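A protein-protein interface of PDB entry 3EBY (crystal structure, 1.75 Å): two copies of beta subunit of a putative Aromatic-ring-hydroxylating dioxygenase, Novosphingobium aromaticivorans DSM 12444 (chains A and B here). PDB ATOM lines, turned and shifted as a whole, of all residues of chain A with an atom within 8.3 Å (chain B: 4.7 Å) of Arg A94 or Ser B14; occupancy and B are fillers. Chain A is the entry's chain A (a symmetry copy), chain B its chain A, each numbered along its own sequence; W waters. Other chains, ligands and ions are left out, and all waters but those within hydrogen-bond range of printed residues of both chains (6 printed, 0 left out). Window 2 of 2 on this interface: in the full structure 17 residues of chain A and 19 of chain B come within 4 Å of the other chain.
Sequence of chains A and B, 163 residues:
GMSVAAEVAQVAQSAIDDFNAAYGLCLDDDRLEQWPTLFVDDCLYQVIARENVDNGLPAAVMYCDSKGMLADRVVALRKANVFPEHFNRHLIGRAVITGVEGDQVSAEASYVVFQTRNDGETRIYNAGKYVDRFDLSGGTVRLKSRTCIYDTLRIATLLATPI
Asp B18 touches Gln A13. Arg A94 touches Ser B14 (NH2 to O, 3.9 Å). Arg A94 touches Asp B17 (CD to O, 3.6 Å). CB of Ala B21 touches O of Arg A94, at 3.6 Å. Ala B21 touches Val A96.
OD1 of Asp B18 lies within salt-bridge range of NE of Arg A94, 2.9 Å away.
Water W3 lies within hydrogen-bond range of OD2 of Asp B17 (2.7 Å), NH1 of Arg A94 (3.1 Å) and NH1 of Arg B94 (3.3 Å). Water W4 lies within hydrogen-bond range of the backbone carbonyl oxygen of Ala A95 (2.7 Å) and the side-chain carboxylate of Asp B18 (2.8 Å). Water W5 lies within hydrogen-bond range of the guanidinium group of Arg A94 (2.8 Å) and the side-chain hydroxyl of Ser B14 (2.8 Å). Water W6 lies within hydrogen-bond range of OD2 of Asp B18 (2.8 Å) and OE1 of Gln A13 (2.8 Å). Water W1 bridges NH1 of Arg B94 (3.1 Å) and NH1 of Arg A94 (3.5 Å). Water W2 bridges NH1 of Arg A94 (3.2 Å) and NH1 of Arg B94 (3.2 Å).
NE2 of Gln A13 sits at hydrogen-bond distance from OD2 of Asp A17, 2.9 Å away. The side-chain carboxylate of Asp B17 lies within salt-bridge range of the guanidinium group of Arg B94, 3.7 Å away. O of Glu A108 is in hydrogen-bond range of N of Val A96 (2.8 Å). The side-chain carboxylate of Asp A17 is in salt-bridge range of the guanidinium group of Arg A94. O of Ala A95 sits at hydrogen-bond distance from NE2 of Gln A13, at 2.9 Å. NE2 of Gln B13 sits at hydrogen-bond distance from OD2 of Asp B17, 2.9 Å away.
Arg A94 touches Ser B14, but with the chains exchanged Ser A14 does not touch Arg B94 (8.3 Å). Arg A94 touches Asp B17, but with the chains exchanged Asp A17 does not touch Arg B94 (7.2 Å). Positions printed for both chains: 10, 13, 14, 16, 17 and 94. Of the 6 pairs that touch across the chains among the printed residues, none has its exchanged pair printed and touching as well.
Of the 11 printed residues of chain B, 4 touch a printed residue of chain A. Printed residues of chain B that touch a printed residue of chain A: Ser B14, Asp B17, Asp B18 and Ala B21. Hydrophobic or aromatic side chains of chain B within 4 Å of the printed part of chain A: Ala B21. Of the 19 printed residues of chain A, 3 touch a printed residue of chain B. Among the printed residues, 6 pairs touch across the chains. Among the printed residues, Asp or Glu carboxylates within 4 Å of a Lys or Arg side-chain nitrogen of the other chain: Arg A94 with Asp B18 (2.9 Å).
Gln A10 touches none of the printed residues of chain B. Of the printed residues of chain B, Arg A94 touches Ser B14 (3.9 Å), Asp B17 (3.6 Å), Asp B18 (2.9 Å) and Ala B21 (3.6 Å). Printed residues of chain B within 4 Å of Val A96: Ala B21. No residue of chain A comes within 4 Å of Ala B15. Printed residues of chain A within 4 Å of Ala B21: Arg A94 (3.6 Å) and Val A96 (3.7 Å). The nearest residue of chain B that does not touch Arg A94 is Arg B94 (4.6 Å).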
ATOM      1  N   ALA A   9      -4.915  -5.952   8.401  1.00  0.00           N
ATOM      2  CA  ALA A   9      -5.701  -7.049   8.977  1.00  0.00           C
ATOM      3  C   ALA A   9      -6.898  -6.510   9.730  1.00  0.00           C
ATOM      4  O   ALA A   9      -8.011  -7.047   9.604  1.00  0.00           O
ATOM      5  CB  ALA A   9      -4.825  -7.878   9.924  1.00  0.00           C
ATOM      6  N   GLN A  10      -6.643  -5.501  10.575  1.00  0.00           N
ATOM      7  CA  GLN A  10      -7.687  -4.822  11.336  1.00  0.00           C
ATOM      8  C   GLN A  10      -8.718  -4.214  10.402  1.00  0.00           C
ATOM      9  O   GLN A  10      -9.922  -4.231  10.700  1.00  0.00           O
ATOM     10  CB  GLN A  10      -7.079  -3.720  12.230  1.00  0.00           C
ATOM     11  CG  GLN A  10      -8.126  -2.833  12.958  1.00  0.00           C
ATOM     12  N   GLN A  13     -10.795  -7.089   8.882  1.00  0.00           N
ATOM     13  CA  GLN A  13     -11.636  -7.637   9.973  1.00  0.00           C
ATOM     14  C   GLN A  13     -12.854  -6.735  10.230  1.00  0.00           C
ATOM     15  O   GLN A  13     -14.003  -7.208  10.274  1.00  0.00           O
ATOM     16  CB  GLN A  13     -10.817  -7.765  11.260  1.00  0.00           C
ATOM     17  CG  GLN A  13     -11.606  -8.372  12.437  1.00  0.00           C
ATOM     18  CD  GLN A  13     -11.818  -9.837  12.278  1.00  0.00           C
ATOM     19  OE1 GLN A  13     -10.867 -10.583  12.113  1.00  0.00           O
ATOM     20  NE2 GLN A  13     -13.094 -10.279  12.344  1.00  0.00           N
ATOM     21  N   SER A  14     -12.603  -5.444  10.407  1.00  0.00           N
ATOM     22  CA  SER A  14     -13.684  -4.501  10.679  1.00  0.00           C
ATOM     23  C   SER A  14     -14.662  -4.413   9.518  1.00  0.00           C
ATOM     24  O   SER A  14     -15.870  -4.306   9.738  1.00  0.00           O
ATOM     25  CB  SER A  14     -13.130  -3.102  10.987  1.00  0.00           C
ATOM     26  OG  SER A  14     -12.389  -3.108  12.175  1.00  0.00           O
ATOM     27  N   ILE A  16     -15.446  -6.685   7.278  1.00  0.00           N
ATOM     28  CA  ILE A  16     -16.244  -7.900   7.189  1.00  0.00           C
ATOM     29  C   ILE A  16     -17.247  -7.967   8.342  1.00  0.00           C
ATOM     30  O   ILE A  16     -18.424  -8.310   8.132  1.00  0.00           O
ATOM     31  CB  ILE A  16     -15.337  -9.168   7.117  1.00  0.00           C
ATOM     32  CG1 ILE A  16     -14.655  -9.219   5.728  1.00  0.00           C
ATOM     33  CG2 ILE A  16     -16.128 -10.429   7.396  1.00  0.00           C
ATOM     34  CD1 ILE A  16     -13.515 -10.183   5.637  1.00  0.00           C
ATOM     35  N   ASP A  17     -16.806  -7.649   9.557  1.00  0.00           N
ATOM     36  CA  ASP A  17     -17.738  -7.645  10.669  1.00  0.00           C
ATOM     37  C   ASP A  17     -18.859  -6.578  10.493  1.00  0.00           C
ATOM     38  O   ASP A  17     -20.021  -6.864  10.750  1.00  0.00           O
ATOM     39  CB  ASP A  17     -17.010  -7.463  12.005  1.00  0.00           C
ATOM     40  CG  ASP A  17     -16.209  -8.704  12.432  1.00  0.00           C
ATOM     41  OD1 ASP A  17     -16.616  -9.844  12.096  1.00  0.00           O
ATOM     42  OD2 ASP A  17     -15.203  -8.525  13.177  1.00  0.00           O
ATOM     43  N   ASN A  20     -21.324  -7.969   7.937  1.00  0.00           N
ATOM     44  CA  ASN A  20     -22.228  -8.988   8.499  1.00  0.00           C
ATOM     45  C   ASN A  20     -23.329  -8.370   9.381  1.00  0.00           C
ATOM     46  O   ASN A  20     -24.482  -8.779   9.296  1.00  0.00           O
ATOM     47  CB  ASN A  20     -21.446 -10.072   9.264  1.00  0.00           C
ATOM     48  CG  ASN A  20     -20.790 -11.089   8.324  1.00  0.00           C
ATOM     49  OD1 ASN A  20     -21.165 -11.181   7.162  1.00  0.00           O
ATOM     50  ND2 ASN A  20     -19.708 -11.735   8.788  1.00  0.00           N
ATOM     51  N   LEU A  91     -28.488 -13.315  14.735  1.00  0.00           N
ATOM     52  CA  LEU A  91     -27.294 -13.011  15.470  1.00  0.00           C
ATOM     53  C   LEU A  91     -26.119 -13.661  14.740  1.00  0.00           C
ATOM     54  O   LEU A  91     -26.117 -14.867  14.480  1.00  0.00           O
ATOM     55  CB  LEU A  91     -27.357 -13.457  16.940  1.00  0.00           C
ATOM     56  CG  LEU A  91     -28.358 -12.740  17.877  1.00  0.00           C
ATOM     57  CD1 LEU A  91     -28.299 -13.431  19.238  1.00  0.00           C
ATOM     58  CD2 LEU A  91     -28.031 -11.264  18.076  1.00  0.00           C
ATOM     59  N   ILE A  92     -25.132 -12.855  14.393  1.00  0.00           N
ATOM     60  CA  ILE A  92     -23.968 -13.321  13.661  1.00  0.00           C
ATOM     61  C   ILE A  92     -22.708 -13.139  14.496  1.00  0.00           C
ATOM     62  O   ILE A  92     -22.420 -12.045  15.031  1.00  0.00           O
ATOM     63  CB  ILE A  92     -23.850 -12.581  12.277  1.00  0.00           C
ATOM     64  CG1 ILE A  92     -25.196 -12.690  11.527  1.00  0.00           C
ATOM     65  CG2 ILE A  92     -22.696 -13.149  11.448  1.00  0.00           C
ATOM     66  CD1 ILE A  92     -25.310 -11.803  10.245  1.00  0.00           C
ATOM     67  N   GLY A  93     -21.939 -14.210  14.614  1.00  0.00           N
ATOM     68  CA  GLY A  93     -20.684 -14.150  15.326  1.00  0.00           C
ATOM     69  C   GLY A  93     -19.623 -13.330  14.622  1.00  0.00           C
ATOM     70  O   GLY A  93     -19.727 -13.026  13.418  1.00  0.00           O
ATOM     71  N   ARG A  94     -18.563 -12.995  15.361  1.00  0.00           N
ATOM     72  CA  ARG A  94     -17.401 -12.339  14.777  1.00  0.00           C
ATOM     73  C   ARG A  94     -16.767 -13.256  13.719  1.00  0.00           C
ATOM     74  O   ARG A  94     -16.682 -14.458  13.902  1.00  0.00           O
ATOM     75  CB  ARG A  94     -16.403 -11.978  15.872  1.00  0.00           C
ATOM     76  CG  ARG A  94     -15.147 -11.262  15.398  1.00  0.00           C
ATOM     77  CD  ARG A  94     -14.293 -10.930  16.603  1.00  0.00           C
ATOM     78  NE  ARG A  94     -13.043 -10.255  16.275  1.00  0.00           N
ATOM     79  CZ  ARG A  94     -12.854  -8.950  16.361  1.00  0.00           C
ATOM     80  NH1 ARG A  94     -13.871  -8.140  16.607  1.00  0.00           N
ATOM     81  NH2 ARG A  94     -11.657  -8.439  16.114  1.00  0.00           N
ATOM     82  N   ALA A  95     -16.310 -12.668  12.625  1.00  0.00           N
ATOM     83  CA  ALA A  95     -15.741 -13.430  11.499  1.00  0.00           C
ATOM     84  C   ALA A  95     -14.315 -13.883  11.789  1.00  0.00           C
ATOM     85  O   ALA A  95     -13.500 -13.117  12.339  1.00  0.00           O
ATOM     86  CB  ALA A  95     -15.772 -12.586  10.196  1.00  0.00           C
ATOM     87  N   VAL A  96     -14.013 -15.108  11.360  1.00  0.00           N
ATOM     88  CA  VAL A  96     -12.640 -15.615  11.307  1.00  0.00           C
ATOM     89  C   VAL A  96     -12.130 -15.578   9.882  1.00  0.00           C
ATOM     90  O   VAL A  96     -12.691 -16.234   8.976  1.00  0.00           O
ATOM     91  CB  VAL A  96     -12.548 -17.075  11.856  1.00  0.00           C
ATOM     92  CG1 VAL A  96     -11.106 -17.578  11.814  1.00  0.00           C
ATOM     93  CG2 VAL A  96     -13.117 -17.157  13.301  1.00  0.00           C
ATOM     94  N   ILE A  97     -11.148 -14.724   9.643  1.00  0.00           N
ATOM     95  CA  ILE A  97     -10.532 -14.624   8.324  1.00  0.00           C
ATOM     96  C   ILE A  97      -9.628 -15.845   8.112  1.00  0.00           C
ATOM     97  O   ILE A  97      -8.712 -16.111   8.916  1.00  0.00           O
ATOM     98  CB  ILE A  97      -9.749 -13.320   8.177  1.00  0.00           C
ATOM     99  CG1 ILE A  97     -10.722 -12.123   8.192  1.00  0.00           C
ATOM    100  CG2 ILE A  97      -8.890 -13.318   6.874  1.00  0.00           C
ATOM    101  CD1 ILE A  97     -10.024 -10.784   8.305  1.00  0.00           C
ATOM    102  N   ALA A 107     -13.521 -15.796   4.583  1.00  0.00           N
ATOM    103  CA  ALA A 107     -13.901 -15.733   6.024  1.00  0.00           C
ATOM    104  C   ALA A 107     -15.053 -16.644   6.330  1.00  0.00           C
ATOM    105  O   ALA A 107     -15.781 -17.056   5.437  1.00  0.00           O
ATOM    106  CB  ALA A 107     -14.234 -14.293   6.455  1.00  0.00           C
ATOM    107  N   GLU A 108     -15.218 -16.931   7.623  1.00  0.00           N
ATOM    108  CA  GLU A 108     -16.333 -17.739   8.124  1.00  0.00           C
ATOM    109  C   GLU A 108     -16.876 -17.112   9.392  1.00  0.00           C
ATOM    110  O   GLU A 108     -16.121 -16.522  10.150  1.00  0.00           O
ATOM    111  CB  GLU A 108     -15.879 -19.172   8.394  1.00  0.00           C
ATOM    112  CG  GLU A 108     -15.177 -19.835   7.194  1.00  0.00           C
ATOM    113  CD  GLU A 108     -14.840 -21.308   7.390  1.00  0.00           C
ATOM    114  OE1 GLU A 108     -15.229 -21.926   8.419  1.00  0.00           O
ATOM    115  OE2 GLU A 108     -14.144 -21.836   6.499  1.00  0.00           O
ATOM    116  N   ALA A 109     -18.199 -17.206   9.593  1.00  0.00           N
ATOM    117  CA  ALA A 109     -18.843 -16.666  10.793  1.00  0.00           C
ATOM    118  C   ALA A 109     -20.066 -17.500  11.144  1.00  0.00           C
ATOM    119  O   ALA A 109     -20.869 -17.838  10.260  1.00  0.00           O
ATOM    120  CB  ALA A 109     -19.231 -15.201  10.565  1.00  0.00           C
ATOM    121  N   SER A 110     -20.191 -17.873  12.420  1.00  0.00           N
ATOM    122  CA  SER A 110     -21.358 -18.582  12.903  1.00  0.00           C
ATOM    123  C   SER A 110     -22.545 -17.650  12.926  1.00  0.00           C
ATOM    124  O   SER A 110     -22.387 -16.452  13.079  1.00  0.00           O
ATOM    125  CB  SER A 110     -21.141 -19.150  14.317  1.00  0.00           C
ATOM    126  OG  SER A 110     -20.178 -20.191  14.261  1.00  0.00           O
ATOM    127  N   TYR A 111     -23.726 -18.217  12.746  1.00  0.00           N
ATOM    128  CA  TYR A 111     -24.988 -17.461  12.818  1.00  0.00           C
ATOM    129  C   TYR A 111     -26.142 -18.317  13.340  1.00  0.00           C
ATOM    130  O   TYR A 111     -26.147 -19.549  13.215  1.00  0.00           O
ATOM    131  CB  TYR A 111     -25.367 -16.885  11.433  1.00  0.00           C
ATOM    132  CG  TYR A 111     -25.868 -17.952  10.455  1.00  0.00           C
ATOM    133  CD1 TYR A 111     -27.168 -18.450  10.532  1.00  0.00           C
ATOM    134  CD2 TYR A 111     -25.007 -18.522   9.520  1.00  0.00           C
ATOM    135  CE1 TYR A 111     -27.597 -19.470   9.676  1.00  0.00           C
ATOM    136  CE2 TYR A 111     -25.430 -19.600   8.693  1.00  0.00           C
ATOM    137  CZ  TYR A 111     -26.715 -20.060   8.789  1.00  0.00           C
ATOM    138  OH  TYR A 111     -27.136 -21.137   8.020  1.00  0.00           O
ATOM    139  N   GLN B  10      -7.137  -1.490  22.458  1.00  0.00           N
ATOM    140  CA  GLN B  10      -7.705  -1.966  21.200  1.00  0.00           C
ATOM    141  C   GLN B  10      -7.039  -3.260  20.770  1.00  0.00           C
ATOM    142  O   GLN B  10      -7.705  -4.164  20.242  1.00  0.00           O
ATOM    143  CB  GLN B  10      -7.541  -0.903  20.092  1.00  0.00           C
ATOM    144  CG  GLN B  10      -7.969  -1.378  18.677  1.00  0.00           C
ATOM    145  N   VAL B  11      -5.720  -3.341  20.969  1.00  0.00           N
ATOM    146  CA  VAL B  11      -4.975  -4.530  20.580  1.00  0.00           C
ATOM    147  C   VAL B  11      -5.402  -5.742  21.413  1.00  0.00           C
ATOM    148  O   VAL B  11      -5.768  -6.770  20.841  1.00  0.00           O
ATOM    149  CB  VAL B  11      -3.434  -4.302  20.635  1.00  0.00           C
ATOM    150  CG1 VAL B  11      -2.674  -5.611  20.391  1.00  0.00           C
ATOM    151  CG2 VAL B  11      -3.023  -3.244  19.597  1.00  0.00           C
ATOM    152  N   ALA B  12      -5.458  -5.603  22.741  1.00  0.00           N
ATOM    153  CA  ALA B  12      -5.918  -6.708  23.599  1.00  0.00           C
ATOM    154  C   ALA B  12      -7.390  -7.083  23.295  1.00  0.00           C
ATOM    155  O   ALA B  12      -7.730  -8.261  23.236  1.00  0.00           O
ATOM    156  CB  ALA B  12      -5.759  -6.364  25.056  1.00  0.00           C
ATOM    157  N   GLN B  13      -8.251  -6.066  23.126  1.00  0.00           N
ATOM    158  CA  GLN B  13      -9.675  -6.315  22.802  1.00  0.00           C
ATOM    159  C   GLN B  13      -9.804  -7.168  21.529  1.00  0.00           C
ATOM    160  O   GLN B  13     -10.514  -8.189  21.511  1.00  0.00           O
ATOM    161  CB  GLN B  13     -10.415  -4.991  22.605  1.00  0.00           C
ATOM    162  CG  GLN B  13     -11.917  -5.159  22.307  1.00  0.00           C
ATOM    163  CD  GLN B  13     -12.691  -5.554  23.518  1.00  0.00           C
ATOM    164  OE1 GLN B  13     -12.640  -4.875  24.530  1.00  0.00           O
ATOM    165  NE2 GLN B  13     -13.445  -6.671  23.420  1.00  0.00           N
ATOM    166  N   SER B  14      -9.128  -6.747  20.468  1.00  0.00           N
ATOM    167  CA  SER B  14      -9.195  -7.468  19.201  1.00  0.00           C
ATOM    168  C   SER B  14      -8.630  -8.875  19.321  1.00  0.00           C
ATOM    169  O   SER B  14      -9.170  -9.809  18.724  1.00  0.00           O
ATOM    170  CB  SER B  14      -8.446  -6.710  18.094  1.00  0.00           C
ATOM    171  OG  SER B  14      -9.072  -5.489  17.814  1.00  0.00           O
ATOM    172  N   ALA B  15      -7.491  -9.007  20.013  1.00  0.00           N
ATOM    173  CA  ALA B  15      -6.850 -10.323  20.224  1.00  0.00           C
ATOM    174  C   ALA B  15      -7.813 -11.317  20.914  1.00  0.00           C
ATOM    175  O   ALA B  15      -7.952 -12.478  20.497  1.00  0.00           O
ATOM    176  CB  ALA B  15      -5.520 -10.148  21.065  1.00  0.00           C
ATOM    177  N   ILE B  16      -8.501 -10.851  21.942  1.00  0.00           N
ATOM    178  CA  ILE B  16      -9.399 -11.698  22.715  1.00  0.00           C
ATOM    179  C   ILE B  16     -10.660 -12.016  21.911  1.00  0.00           C
ATOM    180  O   ILE B  16     -11.118 -13.172  21.889  1.00  0.00           O
ATOM    181  CB  ILE B  16      -9.724 -11.060  24.102  1.00  0.00           C
ATOM    182  CG1 ILE B  16      -8.467 -11.148  25.001  1.00  0.00           C
ATOM    183  CG2 ILE B  16     -10.920 -11.727  24.750  1.00  0.00           C
ATOM    184  CD1 ILE B  16      -8.524 -10.288  26.224  1.00  0.00           C
ATOM    185  N   ASP B  17     -11.233 -11.013  21.250  1.00  0.00           N
ATOM    186  CA  ASP B  17     -12.400 -11.282  20.429  1.00  0.00           C
ATOM    187  C   ASP B  17     -12.078 -12.245  19.247  1.00  0.00           C
ATOM    188  O   ASP B  17     -12.848 -13.156  18.974  1.00  0.00           O
ATOM    189  CB  ASP B  17     -13.036  -9.983  19.922  1.00  0.00           C
ATOM    190  CG  ASP B  17     -13.757  -9.193  21.026  1.00  0.00           C
ATOM    191  OD1 ASP B  17     -14.287  -9.813  21.981  1.00  0.00           O
ATOM    192  OD2 ASP B  17     -13.853  -7.939  20.882  1.00  0.00           O
ATOM    193  N   ASP B  18     -10.905 -12.101  18.630  1.00  0.00           N
ATOM    194  CA  ASP B  18     -10.458 -13.034  17.571  1.00  0.00           C
ATOM    195  C   ASP B  18     -10.288 -14.454  18.140  1.00  0.00           C
ATOM    196  O   ASP B  18     -10.783 -15.434  17.567  1.00  0.00           O
ATOM    197  CB  ASP B  18      -9.111 -12.587  16.992  1.00  0.00           C
ATOM    198  CG  ASP B  18      -9.223 -11.421  16.029  1.00  0.00           C
ATOM    199  OD1 ASP B  18     -10.324 -11.056  15.593  1.00  0.00           O
ATOM    200  OD2 ASP B  18      -8.143 -10.927  15.625  1.00  0.00           O
ATOM    201  N   ALA B  21     -13.776 -16.040  18.652  1.00  0.00           N
ATOM    202  CA  ALA B  21     -14.385 -16.432  17.362  1.00  0.00           C
ATOM    203  C   ALA B  21     -13.813 -17.768  16.867  1.00  0.00           C
ATOM    204  O   ALA B  21     -14.553 -18.689  16.528  1.00  0.00           O
ATOM    205  CB  ALA B  21     -14.201 -15.325  16.318  1.00  0.00           C
ATOM    206  N   ARG B  94     -19.187 -10.205  22.450  1.00  0.00           N
ATOM    207  CA  ARG B  94     -17.966  -9.419  22.565  1.00  0.00           C
ATOM    208  C   ARG B  94     -17.456  -9.465  24.014  1.00  0.00           C
ATOM    209  O   ARG B  94     -18.232  -9.412  24.953  1.00  0.00           O
ATOM    210  CB  ARG B  94     -18.224  -7.986  22.112  1.00  0.00           C
ATOM    211  CG  ARG B  94     -17.019  -7.060  22.158  1.00  0.00           C
ATOM    212  CD  ARG B  94     -17.428  -5.701  21.631  1.00  0.00           C
ATOM    213  NE  ARG B  94     -16.357  -4.713  21.645  1.00  0.00           N
ATOM    214  CZ  ARG B  94     -15.626  -4.388  20.592  1.00  0.00           C
ATOM    215  NH1 ARG B  94     -15.725  -5.080  19.468  1.00  0.00           N
ATOM    216  NH2 ARG B  94     -14.725  -3.422  20.686  1.00  0.00           N
HETATM  217  O   HOH W   1     -16.636  -7.919  18.719  1.00  0.00           O
HETATM  218  O   HOH W   2     -14.143  -4.976  16.715  1.00  0.00           O
HETATM  219  O   HOH W   3     -12.721  -6.445  18.939  1.00  0.00           O
HETATM  220  O   HOH W   4     -11.826 -13.159  14.490  1.00  0.00           O
HETATM  221  O   HOH W   5     -11.099  -5.744  15.922  1.00  0.00           O
HETATM  222  O   HOH W   6      -8.372  -9.712  13.139  1.00  0.00           O
